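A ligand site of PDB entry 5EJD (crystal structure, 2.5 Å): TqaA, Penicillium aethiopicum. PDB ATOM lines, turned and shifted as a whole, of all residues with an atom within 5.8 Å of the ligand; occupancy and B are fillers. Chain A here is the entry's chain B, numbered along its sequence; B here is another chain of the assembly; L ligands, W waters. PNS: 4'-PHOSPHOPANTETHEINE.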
ATOM      1  N   HIS A 169       9.479   3.754   8.237  1.00  0.00           N
ATOM      2  CA  HIS A 169       8.662   2.916   9.118  1.00  0.00           C
ATOM      3  C   HIS A 169       7.294   2.690   8.531  1.00  0.00           C
ATOM      4  O   HIS A 169       6.553   1.809   8.975  1.00  0.00           O
ATOM      5  CB  HIS A 169       8.542   3.527  10.489  1.00  0.00           C
ATOM      6  CG  HIS A 169       8.212   2.547  11.565  1.00  0.00           C
ATOM      7  ND1 HIS A 169       7.436   1.441  11.373  1.00  0.00           N
ATOM      8  CD2 HIS A 169       8.554   2.526  12.875  1.00  0.00           C
ATOM      9  CE1 HIS A 169       7.319   0.773  12.507  1.00  0.00           C
ATOM     10  NE2 HIS A 169       7.982   1.422  13.426  1.00  0.00           N
ATOM     11  N   TRP A 172       7.469  -1.176   7.354  1.00  0.00           N
ATOM     12  CA  TRP A 172       7.683  -2.356   8.169  1.00  0.00           C
ATOM     13  C   TRP A 172       6.999  -2.216   9.509  1.00  0.00           C
ATOM     14  O   TRP A 172       6.638  -1.130   9.901  1.00  0.00           O
ATOM     15  CB  TRP A 172       9.207  -2.586   8.393  1.00  0.00           C
ATOM     16  CG  TRP A 172       9.878  -1.526   9.182  1.00  0.00           C
ATOM     17  CD1 TRP A 172      10.427  -0.408   8.696  1.00  0.00           C
ATOM     18  CD2 TRP A 172      10.065  -1.474  10.597  1.00  0.00           C
ATOM     19  NE1 TRP A 172      10.978   0.373   9.726  1.00  0.00           N
ATOM     20  CE2 TRP A 172      10.742  -0.275  10.902  1.00  0.00           C
ATOM     21  CE3 TRP A 172       9.724  -2.331  11.647  1.00  0.00           C
ATOM     22  CZ2 TRP A 172      11.076   0.092  12.208  1.00  0.00           C
ATOM     23  CZ3 TRP A 172      10.046  -1.965  12.972  1.00  0.00           C
ATOM     24  CH2 TRP A 172      10.690  -0.756  13.229  1.00  0.00           C
ATOM     25  N   ASP A 173       6.863  -3.323  10.204  1.00  0.00           N
ATOM     26  CA  ASP A 173       6.511  -3.305  11.601  1.00  0.00           C
ATOM     27  C   ASP A 173       7.185  -4.416  12.386  1.00  0.00           C
ATOM     28  O   ASP A 173       7.917  -5.223  11.812  1.00  0.00           O
ATOM     29  CB  ASP A 173       5.004  -3.375  11.735  1.00  0.00           C
ATOM     30  CG  ASP A 173       4.405  -4.590  11.100  1.00  0.00           C
ATOM     31  OD1 ASP A 173       5.075  -5.671  10.957  1.00  0.00           O
ATOM     32  OD2 ASP A 173       3.187  -4.468  10.758  1.00  0.00           O
ATOM     33  N   GLY A 174       6.931  -4.481  13.680  1.00  0.00           N
ATOM     34  CA  GLY A 174       7.685  -5.365  14.549  1.00  0.00           C
ATOM     35  C   GLY A 174       7.461  -6.838  14.295  1.00  0.00           C
ATOM     36  O   GLY A 174       8.360  -7.653  14.456  1.00  0.00           O
ATOM     37  N   VAL A 175       6.246  -7.181  13.875  1.00  0.00           N
ATOM     38  CA  VAL A 175       5.959  -8.544  13.536  1.00  0.00           C
ATOM     39  C   VAL A 175       6.728  -9.004  12.296  1.00  0.00           C
ATOM     40  O   VAL A 175       7.168 -10.120  12.236  1.00  0.00           O
ATOM     41  CB  VAL A 175       4.471  -8.696  13.265  1.00  0.00           C
ATOM     42  CG1 VAL A 175       4.179 -10.072  12.691  1.00  0.00           C
ATOM     43  CG2 VAL A 175       3.696  -8.463  14.545  1.00  0.00           C
ATOM     44  N   THR A 273      -2.094 -10.750  30.548  1.00  0.00           N
ATOM     45  CA  THR A 273      -0.883 -10.527  29.764  1.00  0.00           C
ATOM     46  C   THR A 273      -0.137  -9.299  30.275  1.00  0.00           C
ATOM     47  O   THR A 273      -0.682  -8.476  31.007  1.00  0.00           O
ATOM     48  CB  THR A 273      -1.192 -10.284  28.299  1.00  0.00           C
ATOM     49  OG1 THR A 273      -1.901  -9.050  28.130  1.00  0.00           O
ATOM     50  CG2 THR A 273      -2.033 -11.419  27.757  1.00  0.00           C
ATOM     51  N   MET A 274       1.138  -9.228  29.919  1.00  0.00           N
ATOM     52  CA  MET A 274       1.978  -8.124  30.307  1.00  0.00           C
ATOM     53  C   MET A 274       1.431  -6.818  29.751  1.00  0.00           C
ATOM     54  O   MET A 274       1.461  -5.795  30.394  1.00  0.00           O
ATOM     55  CB  MET A 274       3.375  -8.383  29.801  1.00  0.00           C
ATOM     56  CG  MET A 274       4.380  -7.300  30.154  1.00  0.00           C
ATOM     57  SD  MET A 274       4.765  -7.327  31.891  1.00  0.00           S
ATOM     58  CE  MET A 274       5.931  -8.727  31.893  1.00  0.00           C
ATOM     59  N   ALA A 275       0.962  -6.858  28.513  1.00  0.00           N
ATOM     60  CA  ALA A 275       0.425  -5.667  27.893  1.00  0.00           C
ATOM     61  C   ALA A 275      -0.718  -5.104  28.698  1.00  0.00           C
ATOM     62  O   ALA A 275      -0.825  -3.901  28.843  1.00  0.00           O
ATOM     63  CB  ALA A 275      -0.071  -5.983  26.477  1.00  0.00           C
ATOM     64  N   THR A 276      -1.578  -5.984  29.194  1.00  0.00           N
ATOM     65  CA  THR A 276      -2.705  -5.563  30.007  1.00  0.00           C
ATOM     66  C   THR A 276      -2.208  -4.847  31.272  1.00  0.00           C
ATOM     67  O   THR A 276      -2.691  -3.782  31.656  1.00  0.00           O
ATOM     68  CB  THR A 276      -3.572  -6.764  30.405  1.00  0.00           C
ATOM     69  OG1 THR A 276      -4.242  -7.278  29.242  1.00  0.00           O
ATOM     70  CG2 THR A 276      -4.635  -6.360  31.442  1.00  0.00           C
ATOM     71  N   LYS A 279      -1.061  -1.372  30.422  1.00  0.00           N
ATOM     72  CA  LYS A 279      -2.148  -0.459  30.077  1.00  0.00           C
ATOM     73  C   LYS A 279      -3.028  -0.097  31.279  1.00  0.00           C
ATOM     74  O   LYS A 279      -3.493   1.029  31.386  1.00  0.00           O
ATOM     75  CB  LYS A 279      -2.956  -1.018  28.949  1.00  0.00           C
ATOM     76  CG  LYS A 279      -2.201  -0.825  27.662  1.00  0.00           C
ATOM     77  CD  LYS A 279      -2.591  -1.735  26.545  1.00  0.00           C
ATOM     78  CE  LYS A 279      -1.503  -1.643  25.458  1.00  0.00           C
ATOM     79  NZ  LYS A 279      -1.770  -2.566  24.332  1.00  0.00           N
ATOM     80  N   HIS A 299      -3.520   3.286  21.897  1.00  0.00           N
ATOM     81  CA  HIS A 299      -2.554   2.216  21.986  1.00  0.00           C
ATOM     82  C   HIS A 299      -2.345   1.562  20.664  1.00  0.00           C
ATOM     83  O   HIS A 299      -3.149   1.687  19.748  1.00  0.00           O
ATOM     84  CB  HIS A 299      -2.925   1.214  23.088  1.00  0.00           C
ATOM     85  CG  HIS A 299      -4.043   0.300  22.725  1.00  0.00           C
ATOM     86  ND1 HIS A 299      -4.042  -1.028  23.064  1.00  0.00           N
ATOM     87  CD2 HIS A 299      -5.201   0.516  22.059  1.00  0.00           C
ATOM     88  CE1 HIS A 299      -5.130  -1.608  22.604  1.00  0.00           C
ATOM     89  NE2 HIS A 299      -5.850  -0.699  21.982  1.00  0.00           N
ATOM     90  N   THR A 300      -1.205   0.889  20.551  1.00  0.00           N
ATOM     91  CA  THR A 300      -0.734   0.313  19.282  1.00  0.00           C
ATOM     92  C   THR A 300      -1.133  -1.134  19.199  1.00  0.00           C
ATOM     93  O   THR A 300      -0.926  -1.891  20.125  1.00  0.00           O
ATOM     94  CB  THR A 300       0.775   0.381  19.202  1.00  0.00           C
ATOM     95  OG1 THR A 300       1.177   1.753  19.344  1.00  0.00           O
ATOM     96  CG2 THR A 300       1.231  -0.134  17.867  1.00  0.00           C
ATOM     97  N   VAL A 301      -1.804  -1.480  18.116  1.00  0.00           N
ATOM     98  CA  VAL A 301      -2.229  -2.845  17.891  1.00  0.00           C
ATOM     99  C   VAL A 301      -1.629  -3.314  16.562  1.00  0.00           C
ATOM    100  O   VAL A 301      -1.306  -2.506  15.716  1.00  0.00           O
ATOM    101  CB  VAL A 301      -3.754  -2.987  17.871  1.00  0.00           C
ATOM    102  CG1 VAL A 301      -4.333  -2.619  19.227  1.00  0.00           C
ATOM    103  CG2 VAL A 301      -4.374  -2.154  16.757  1.00  0.00           C
ATOM    104  N   ASN A 302      -1.502  -4.636  16.401  1.00  0.00           N
ATOM    105  CA  ASN A 302      -0.716  -5.165  15.318  1.00  0.00           C
ATOM    106  C   ASN A 302      -1.428  -5.231  14.008  1.00  0.00           C
ATOM    107  O   ASN A 302      -0.789  -5.324  12.940  1.00  0.00           O
ATOM    108  CB  ASN A 302      -0.113  -6.504  15.692  1.00  0.00           C
ATOM    109  CG  ASN A 302      -1.150  -7.558  15.972  1.00  0.00           C
ATOM    110  OD1 ASN A 302      -1.843  -8.000  15.079  1.00  0.00           O
ATOM    111  ND2 ASN A 302      -1.257  -7.975  17.225  1.00  0.00           N
ATOM    112  N   GLY A 303      -2.752  -5.192  14.047  1.00  0.00           N
ATOM    113  CA  GLY A 303      -3.531  -5.100  12.808  1.00  0.00           C
ATOM    114  C   GLY A 303      -3.614  -6.359  11.950  1.00  0.00           C
ATOM    115  O   GLY A 303      -4.062  -6.302  10.790  1.00  0.00           O
ATOM    116  N   LEU A 319       0.440  -1.984  11.555  1.00  0.00           N
ATOM    117  CA  LEU A 319       0.135  -1.357  12.838  1.00  0.00           C
ATOM    118  C   LEU A 319      -1.010  -0.401  12.768  1.00  0.00           C
ATOM    119  O   LEU A 319      -1.210   0.267  11.760  1.00  0.00           O
ATOM    120  CB  LEU A 319       1.297  -0.458  13.296  1.00  0.00           C
ATOM    121  CG  LEU A 319       2.563  -1.112  13.665  1.00  0.00           C
ATOM    122  CD1 LEU A 319       3.501  -0.042  14.177  1.00  0.00           C
ATOM    123  CD2 LEU A 319       2.321  -2.167  14.720  1.00  0.00           C
ATOM    124  N   GLN A 345      -8.126  -5.719  30.095  1.00  0.00           N
ATOM    125  CA  GLN A 345      -7.951  -6.753  29.126  1.00  0.00           C
ATOM    126  C   GLN A 345      -9.174  -7.001  28.245  1.00  0.00           C
ATOM    127  O   GLN A 345      -9.066  -7.158  27.016  1.00  0.00           O
ATOM    128  CB  GLN A 345      -7.557  -8.055  29.809  1.00  0.00           C
ATOM    129  CG  GLN A 345      -7.067  -9.121  28.829  1.00  0.00           C
ATOM    130  CD  GLN A 345      -6.059 -10.075  29.482  1.00  0.00           C
ATOM    131  OE1 GLN A 345      -4.868  -9.719  29.782  1.00  0.00           O
ATOM    132  NE2 GLN A 345      -6.495 -11.307  29.662  1.00  0.00           N
ATOM    133  N   TYR A 348      -9.644  -4.427  25.529  1.00  0.00           N
ATOM    134  CA  TYR A 348      -8.789  -4.663  24.367  1.00  0.00           C
ATOM    135  C   TYR A 348      -9.395  -5.760  23.545  1.00  0.00           C
ATOM    136  O   TYR A 348      -9.613  -5.542  22.356  1.00  0.00           O
ATOM    137  CB  TYR A 348      -7.354  -5.015  24.776  1.00  0.00           C
ATOM    138  CG  TYR A 348      -6.583  -5.751  23.712  1.00  0.00           C
ATOM    139  CD1 TYR A 348      -6.319  -5.173  22.490  1.00  0.00           C
ATOM    140  CD2 TYR A 348      -6.112  -7.032  23.943  1.00  0.00           C
ATOM    141  CE1 TYR A 348      -5.623  -5.854  21.522  1.00  0.00           C
ATOM    142  CE2 TYR A 348      -5.383  -7.695  22.991  1.00  0.00           C
ATOM    143  CZ  TYR A 348      -5.154  -7.131  21.800  1.00  0.00           C
ATOM    144  OH  TYR A 348      -4.406  -7.846  20.864  1.00  0.00           O
ATOM    145  N   GLU A 355     -10.137  -3.576  15.080  1.00  0.00           N
ATOM    146  CA  GLU A 355      -8.969  -2.731  15.389  1.00  0.00           C
ATOM    147  C   GLU A 355      -8.221  -2.327  14.138  1.00  0.00           C
ATOM    148  O   GLU A 355      -7.245  -1.609  14.220  1.00  0.00           O
ATOM    149  CB  GLU A 355      -8.000  -3.489  16.345  1.00  0.00           C
ATOM    150  CG  GLU A 355      -7.349  -4.727  15.705  1.00  0.00           C
ATOM    151  CD  GLU A 355      -6.209  -5.394  16.512  1.00  0.00           C
ATOM    152  OE1 GLU A 355      -6.198  -5.279  17.793  1.00  0.00           O
ATOM    153  OE2 GLU A 355      -5.313  -6.046  15.863  1.00  0.00           O
ATOM    154  N   GLN A 380       2.629   1.646  23.597  1.00  0.00           N
ATOM    155  CA  GLN A 380       3.019   0.468  22.801  1.00  0.00           C
ATOM    156  C   GLN A 380       3.706  -0.538  23.632  1.00  0.00           C
ATOM    157  O   GLN A 380       4.887  -0.329  23.961  1.00  0.00           O
ATOM    158  CB  GLN A 380       4.148   0.648  21.803  1.00  0.00           C
ATOM    159  CG  GLN A 380       3.901   1.575  20.722  1.00  0.00           C
ATOM    160  CD  GLN A 380       4.534   1.198  19.404  1.00  0.00           C
ATOM    161  OE1 GLN A 380       5.605   0.560  19.253  1.00  0.00           O
ATOM    162  NE2 GLN A 380       3.900   1.690  18.430  1.00  0.00           N
ATOM    163  N   HIS A 381       3.101  -1.674  23.789  1.00  0.00           N
ATOM    164  CA  HIS A 381       3.833  -2.699  24.401  1.00  0.00           C
ATOM    165  C   HIS A 381       4.575  -3.505  23.302  1.00  0.00           C
ATOM    166  O   HIS A 381       3.971  -3.993  22.358  1.00  0.00           O
ATOM    167  CB  HIS A 381       2.889  -3.570  25.224  1.00  0.00           C
ATOM    168  CG  HIS A 381       3.604  -4.668  25.919  1.00  0.00           C
ATOM    169  ND1 HIS A 381       4.522  -4.439  26.917  1.00  0.00           N
ATOM    170  CD2 HIS A 381       3.588  -6.007  25.722  1.00  0.00           C
ATOM    171  CE1 HIS A 381       4.989  -5.592  27.363  1.00  0.00           C
ATOM    172  NE2 HIS A 381       4.458  -6.558  26.652  1.00  0.00           N
ATOM    173  N   GLN A 382       5.876  -3.713  23.489  1.00  0.00           N
ATOM    174  CA  GLN A 382       6.708  -4.360  22.506  1.00  0.00           C
ATOM    175  C   GLN A 382       6.888  -5.878  22.711  1.00  0.00           C
ATOM    176  O   GLN A 382       7.964  -6.342  22.966  1.00  0.00           O
ATOM    177  CB  GLN A 382       8.079  -3.736  22.543  1.00  0.00           C
ATOM    178  CG  GLN A 382       8.086  -2.237  22.479  1.00  0.00           C
ATOM    179  CD  GLN A 382       7.866  -1.728  21.057  1.00  0.00           C
ATOM    180  OE1 GLN A 382       6.957  -2.155  20.372  1.00  0.00           O
ATOM    181  NE2 GLN A 382       8.635  -0.733  20.674  1.00  0.00           N
ATOM    182  N   ASN A 383       5.818  -6.646  22.554  1.00  0.00           N
ATOM    183  CA  ASN A 383       5.911  -8.061  22.649  1.00  0.00           C
ATOM    184  C   ASN A 383       6.202  -8.677  21.311  1.00  0.00           C
ATOM    185  O   ASN A 383       5.566  -9.623  20.862  1.00  0.00           O
ATOM    186  CB  ASN A 383       4.673  -8.660  23.336  1.00  0.00           C
ATOM    187  CG  ASN A 383       3.370  -8.176  22.789  1.00  0.00           C
ATOM    188  OD1 ASN A 383       3.306  -7.268  21.963  1.00  0.00           O
ATOM    189  ND2 ASN A 383       2.296  -8.752  23.284  1.00  0.00           N
ATOM    190  N   ILE A 384       7.283  -8.223  20.719  1.00  0.00           N
ATOM    191  CA  ILE A 384       7.766  -8.682  19.422  1.00  0.00           C
ATOM    192  C   ILE A 384       9.269  -8.956  19.575  1.00  0.00           C
ATOM    193  O   ILE A 384       9.845  -8.691  20.614  1.00  0.00           O
ATOM    194  CB  ILE A 384       7.654  -7.571  18.417  1.00  0.00           C
ATOM    195  CG1 ILE A 384       8.142  -6.281  19.111  1.00  0.00           C
ATOM    196  CG2 ILE A 384       6.237  -7.440  17.973  1.00  0.00           C
ATOM    197  CD1 ILE A 384       8.473  -5.174  18.190  1.00  0.00           C
ATOM    198  N   HIS B  39       1.427 -15.099  24.176  1.00  0.00           N
ATOM    199  CA  HIS B  39       0.806 -13.801  24.336  1.00  0.00           C
ATOM    200  C   HIS B  39       0.024 -13.406  23.058  1.00  0.00           C
ATOM    201  O   HIS B  39      -0.220 -14.237  22.201  1.00  0.00           O
ATOM    202  CB  HIS B  39       1.826 -12.735  24.751  1.00  0.00           C
ATOM    203  CG  HIS B  39       2.982 -12.622  23.837  1.00  0.00           C
ATOM    204  ND1 HIS B  39       2.859 -12.639  22.467  1.00  0.00           N
ATOM    205  CD2 HIS B  39       4.302 -12.509  24.104  1.00  0.00           C
ATOM    206  CE1 HIS B  39       4.061 -12.577  21.923  1.00  0.00           C
ATOM    207  NE2 HIS B  39       4.953 -12.478  22.887  1.00  0.00           N
ATOM    208  N   SER B  40      -0.399 -12.148  22.982  1.00  0.00           N
ATOM    209  CA  SER B  40      -1.318 -11.706  21.963  1.00  0.00           C
ATOM    210  C   SER B  40      -0.747 -11.948  20.566  1.00  0.00           C
ATOM    211  O   SER B  40      -1.479 -12.286  19.672  1.00  0.00           O
ATOM    212  CB  SER B  40      -1.657 -10.226  22.132  1.00  0.00           C
ATOM    213  OG  SER B  40      -2.069  -9.889  23.443  1.00  0.00           O
ATOM    214  N   ILE B  41       0.539 -11.729  20.366  1.00  0.00           N
ATOM    215  CA  ILE B  41       1.153 -11.889  19.066  1.00  0.00           C
ATOM    216  C   ILE B  41       1.281 -13.348  18.656  1.00  0.00           C
ATOM    217  O   ILE B  41       1.015 -13.683  17.503  1.00  0.00           O
ATOM    218  CB  ILE B  41       2.446 -11.103  18.972  1.00  0.00           C
ATOM    219  CG1 ILE B  41       2.008  -9.653  18.848  1.00  0.00           C
ATOM    220  CG2 ILE B  41       3.253 -11.526  17.762  1.00  0.00           C
ATOM    221  CD1 ILE B  41       3.027  -8.663  18.478  1.00  0.00           C
ATOM    222  N   PHE B  63      -8.357 -15.786  23.749  1.00  0.00           N
ATOM    223  CA  PHE B  63      -8.541 -15.177  25.090  1.00  0.00           C
ATOM    224  C   PHE B  63      -9.761 -15.745  25.853  1.00  0.00           C
ATOM    225  O   PHE B  63      -9.723 -15.854  27.063  1.00  0.00           O
ATOM    226  CB  PHE B  63      -8.658 -13.646  25.024  1.00  0.00           C
ATOM    227  CG  PHE B  63      -7.333 -12.935  24.892  1.00  0.00           C
ATOM    228  CD1 PHE B  63      -6.687 -12.443  26.003  1.00  0.00           C
ATOM    229  CD2 PHE B  63      -6.762 -12.743  23.628  1.00  0.00           C
ATOM    230  CE1 PHE B  63      -5.478 -11.786  25.888  1.00  0.00           C
ATOM    231  CE2 PHE B  63      -5.569 -12.083  23.508  1.00  0.00           C
ATOM    232  CZ  PHE B  63      -4.919 -11.594  24.643  1.00  0.00           C
HETATM  233  O23 PNS L   1      -0.092  -9.918  24.888  1.00  0.00           O
HETATM  234  P24 PNS L   1      -1.214  -9.013  24.453  1.00  0.00           P
HETATM  235  O26 PNS L   1      -2.233  -8.691  25.468  1.00  0.00           O
HETATM  236  O27 PNS L   1      -0.707  -7.809  23.470  1.00  0.00           O
HETATM  237  C28 PNS L   1      -1.394  -6.656  23.050  1.00  0.00           C
HETATM  238  C29 PNS L   1      -0.609  -5.724  22.014  1.00  0.00           C
HETATM  239  C30 PNS L   1       0.280  -5.208  23.097  1.00  0.00           C
HETATM  240  C31 PNS L   1      -1.931  -5.009  21.695  1.00  0.00           C
HETATM  241  C32 PNS L   1      -0.024  -6.751  20.998  1.00  0.00           C
HETATM  242  O33 PNS L   1      -1.121  -7.613  20.502  1.00  0.00           O
HETATM  243  C34 PNS L   1       0.392  -5.922  19.806  1.00  0.00           C
HETATM  244  O35 PNS L   1      -0.429  -5.654  18.912  1.00  0.00           O
HETATM  245  N36 PNS L   1       1.437  -5.244  19.457  1.00  0.00           N
HETATM  246  C37 PNS L   1       2.694  -5.019  20.007  1.00  0.00           C
HETATM  247  C38 PNS L   1       3.770  -5.121  18.936  1.00  0.00           C
HETATM  248  C39 PNS L   1       4.060  -3.911  18.096  1.00  0.00           C
HETATM  249  O40 PNS L   1       3.297  -3.605  17.224  1.00  0.00           O
HETATM  250  N41 PNS L   1       5.235  -3.304  18.317  1.00  0.00           N
HETATM  251  C42 PNS L   1       5.689  -2.137  17.620  1.00  0.00           C
HETATM  252  C43 PNS L   1       5.941  -2.394  16.168  1.00  0.00           C
HETATM  253  S44 PNS L   1       7.434  -1.532  15.617  1.00  0.00           S
HETATM  254  O   HOH W   1      -3.861  -6.626  26.499  1.00  0.00           O
HETATM  255  O   HOH W   2       3.952  -4.963  14.517  1.00  0.00           O
HETATM  256  O   HOH W   3       1.814  -9.331  26.685  1.00  0.00           O
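Water W1 lies within hydrogen-bond range of an oxygen (O26) of the ligand and the side-chain hydroxyl (OG1) of Thr 276. Water W2 lies within hydrogen-bond range of O40 of the ligand (3.1 Å), N of Gly 174 (3.1 Å) and N of Val 175 (3.3 Å).
The backbone NH of Asn 302 lies within hydrogen-bond range of an oxygen (O35) of the ligand, at 2.9 Å. An oxygen (O35) of the ligand lies within hydrogen-bond range of the side-chain amide nitrogen of Asn 302, at 3.0 Å. A nitrogen (N41) of the ligand is in hydrogen-bond range of the side-chain amide oxygen (OE1) of Gln 382, 2.9 Å away. An oxygen (O26) of the ligand is in hydrogen-bond range of the side-chain hydroxyl (OG1) of Thr 273 (2.7 Å). A sulfur (S44) of the ligand lies close to a ring nitrogen (NE2) of His 169 (3.7 Å). An oxygen (O23) of the ligand lies within hydrogen-bond range of the side-chain amide nitrogen (ND2) of Asn 383 (3.1 Å). OH of Tyr 348 is in hydrogen-bond range of O33 of the ligand. A sulfur (S44) of the ligand lies close to the backbone NH (N) of Gly 174 (3.6 Å). The side-chain hydroxyl (OG) of Ser 40 of chain B is bonded to a phosphorus (P24) of the ligand, at 1.6 Å. The backbone NH (N) of Ser 40 of chain B sits at hydrogen-bond distance from an oxygen (O23) of the ligand, at 2.9 Å.
The side-chain amide oxygen (OE1) of Gln 382 lies close to the side-chain amide oxygen (OE1) of Gln 380 (3.2 Å). The backbone carbonyl oxygen (O) of His 381 sits close to the side-chain amide oxygen (OD1) of Asn 383. The side-chain amide nitrogen (NE2) of Gln 380 sits at hydrogen-bond distance from the side-chain hydroxyl (OG1) of Thr 300, at 2.9 Å. N of Thr 273 lies within hydrogen-bond range of OE1 of Gln 345 (3.1 Å). O of Trp 172 sits at hydrogen-bond distance from ND1 of His 169, 3.1 Å away. The side-chain hydroxyl (OG1) of Thr 276 is in hydrogen-bond range of the side-chain hydroxyl (OG1) of Thr 273 (3.1 Å). NZ of Lys 279 is in hydrogen-bond range of ND1 of His 299 (3.0 Å). A ring nitrogen (ND1) of His 39 of chain B sits close to the backbone NH (N) of Ile 41 of chain B, at 3.3 Å.
Trp 172 touches the ligand (CZ3 to S44, 3.7 Å). Ala 275 touches the ligand. Lys 279 touches the ligand. Thr 300 touches the ligand (O to C31, 3.6 Å). CA of Val 301 touches O35 of the ligand, at 3.5 Å. Leu 319 touches the ligand (CD2 to O40, 3.0 Å). Gln 380 touches the ligand. His 381 touches the ligand. Ile 384 touches the ligand (CG2 to C38, 3.5 Å). CB of His 39 of chain B touches O23 of the ligand, 3.4 Å away. Ile 41 of chain B touches the ligand. Hydrophobic or aromatic side chains within 4 Å of the ligand: His 169, Trp 172, Ala 275, Leu 319, Tyr 348, His 381, Ile 384, His 39 of chain B and Ile 41 of chain B. Of the 28 residues printed, 19 come within 4 Å of the ligand. The nearest printed residue that does not touch the ligand is Phe 63 of chain B (4.04 Å).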
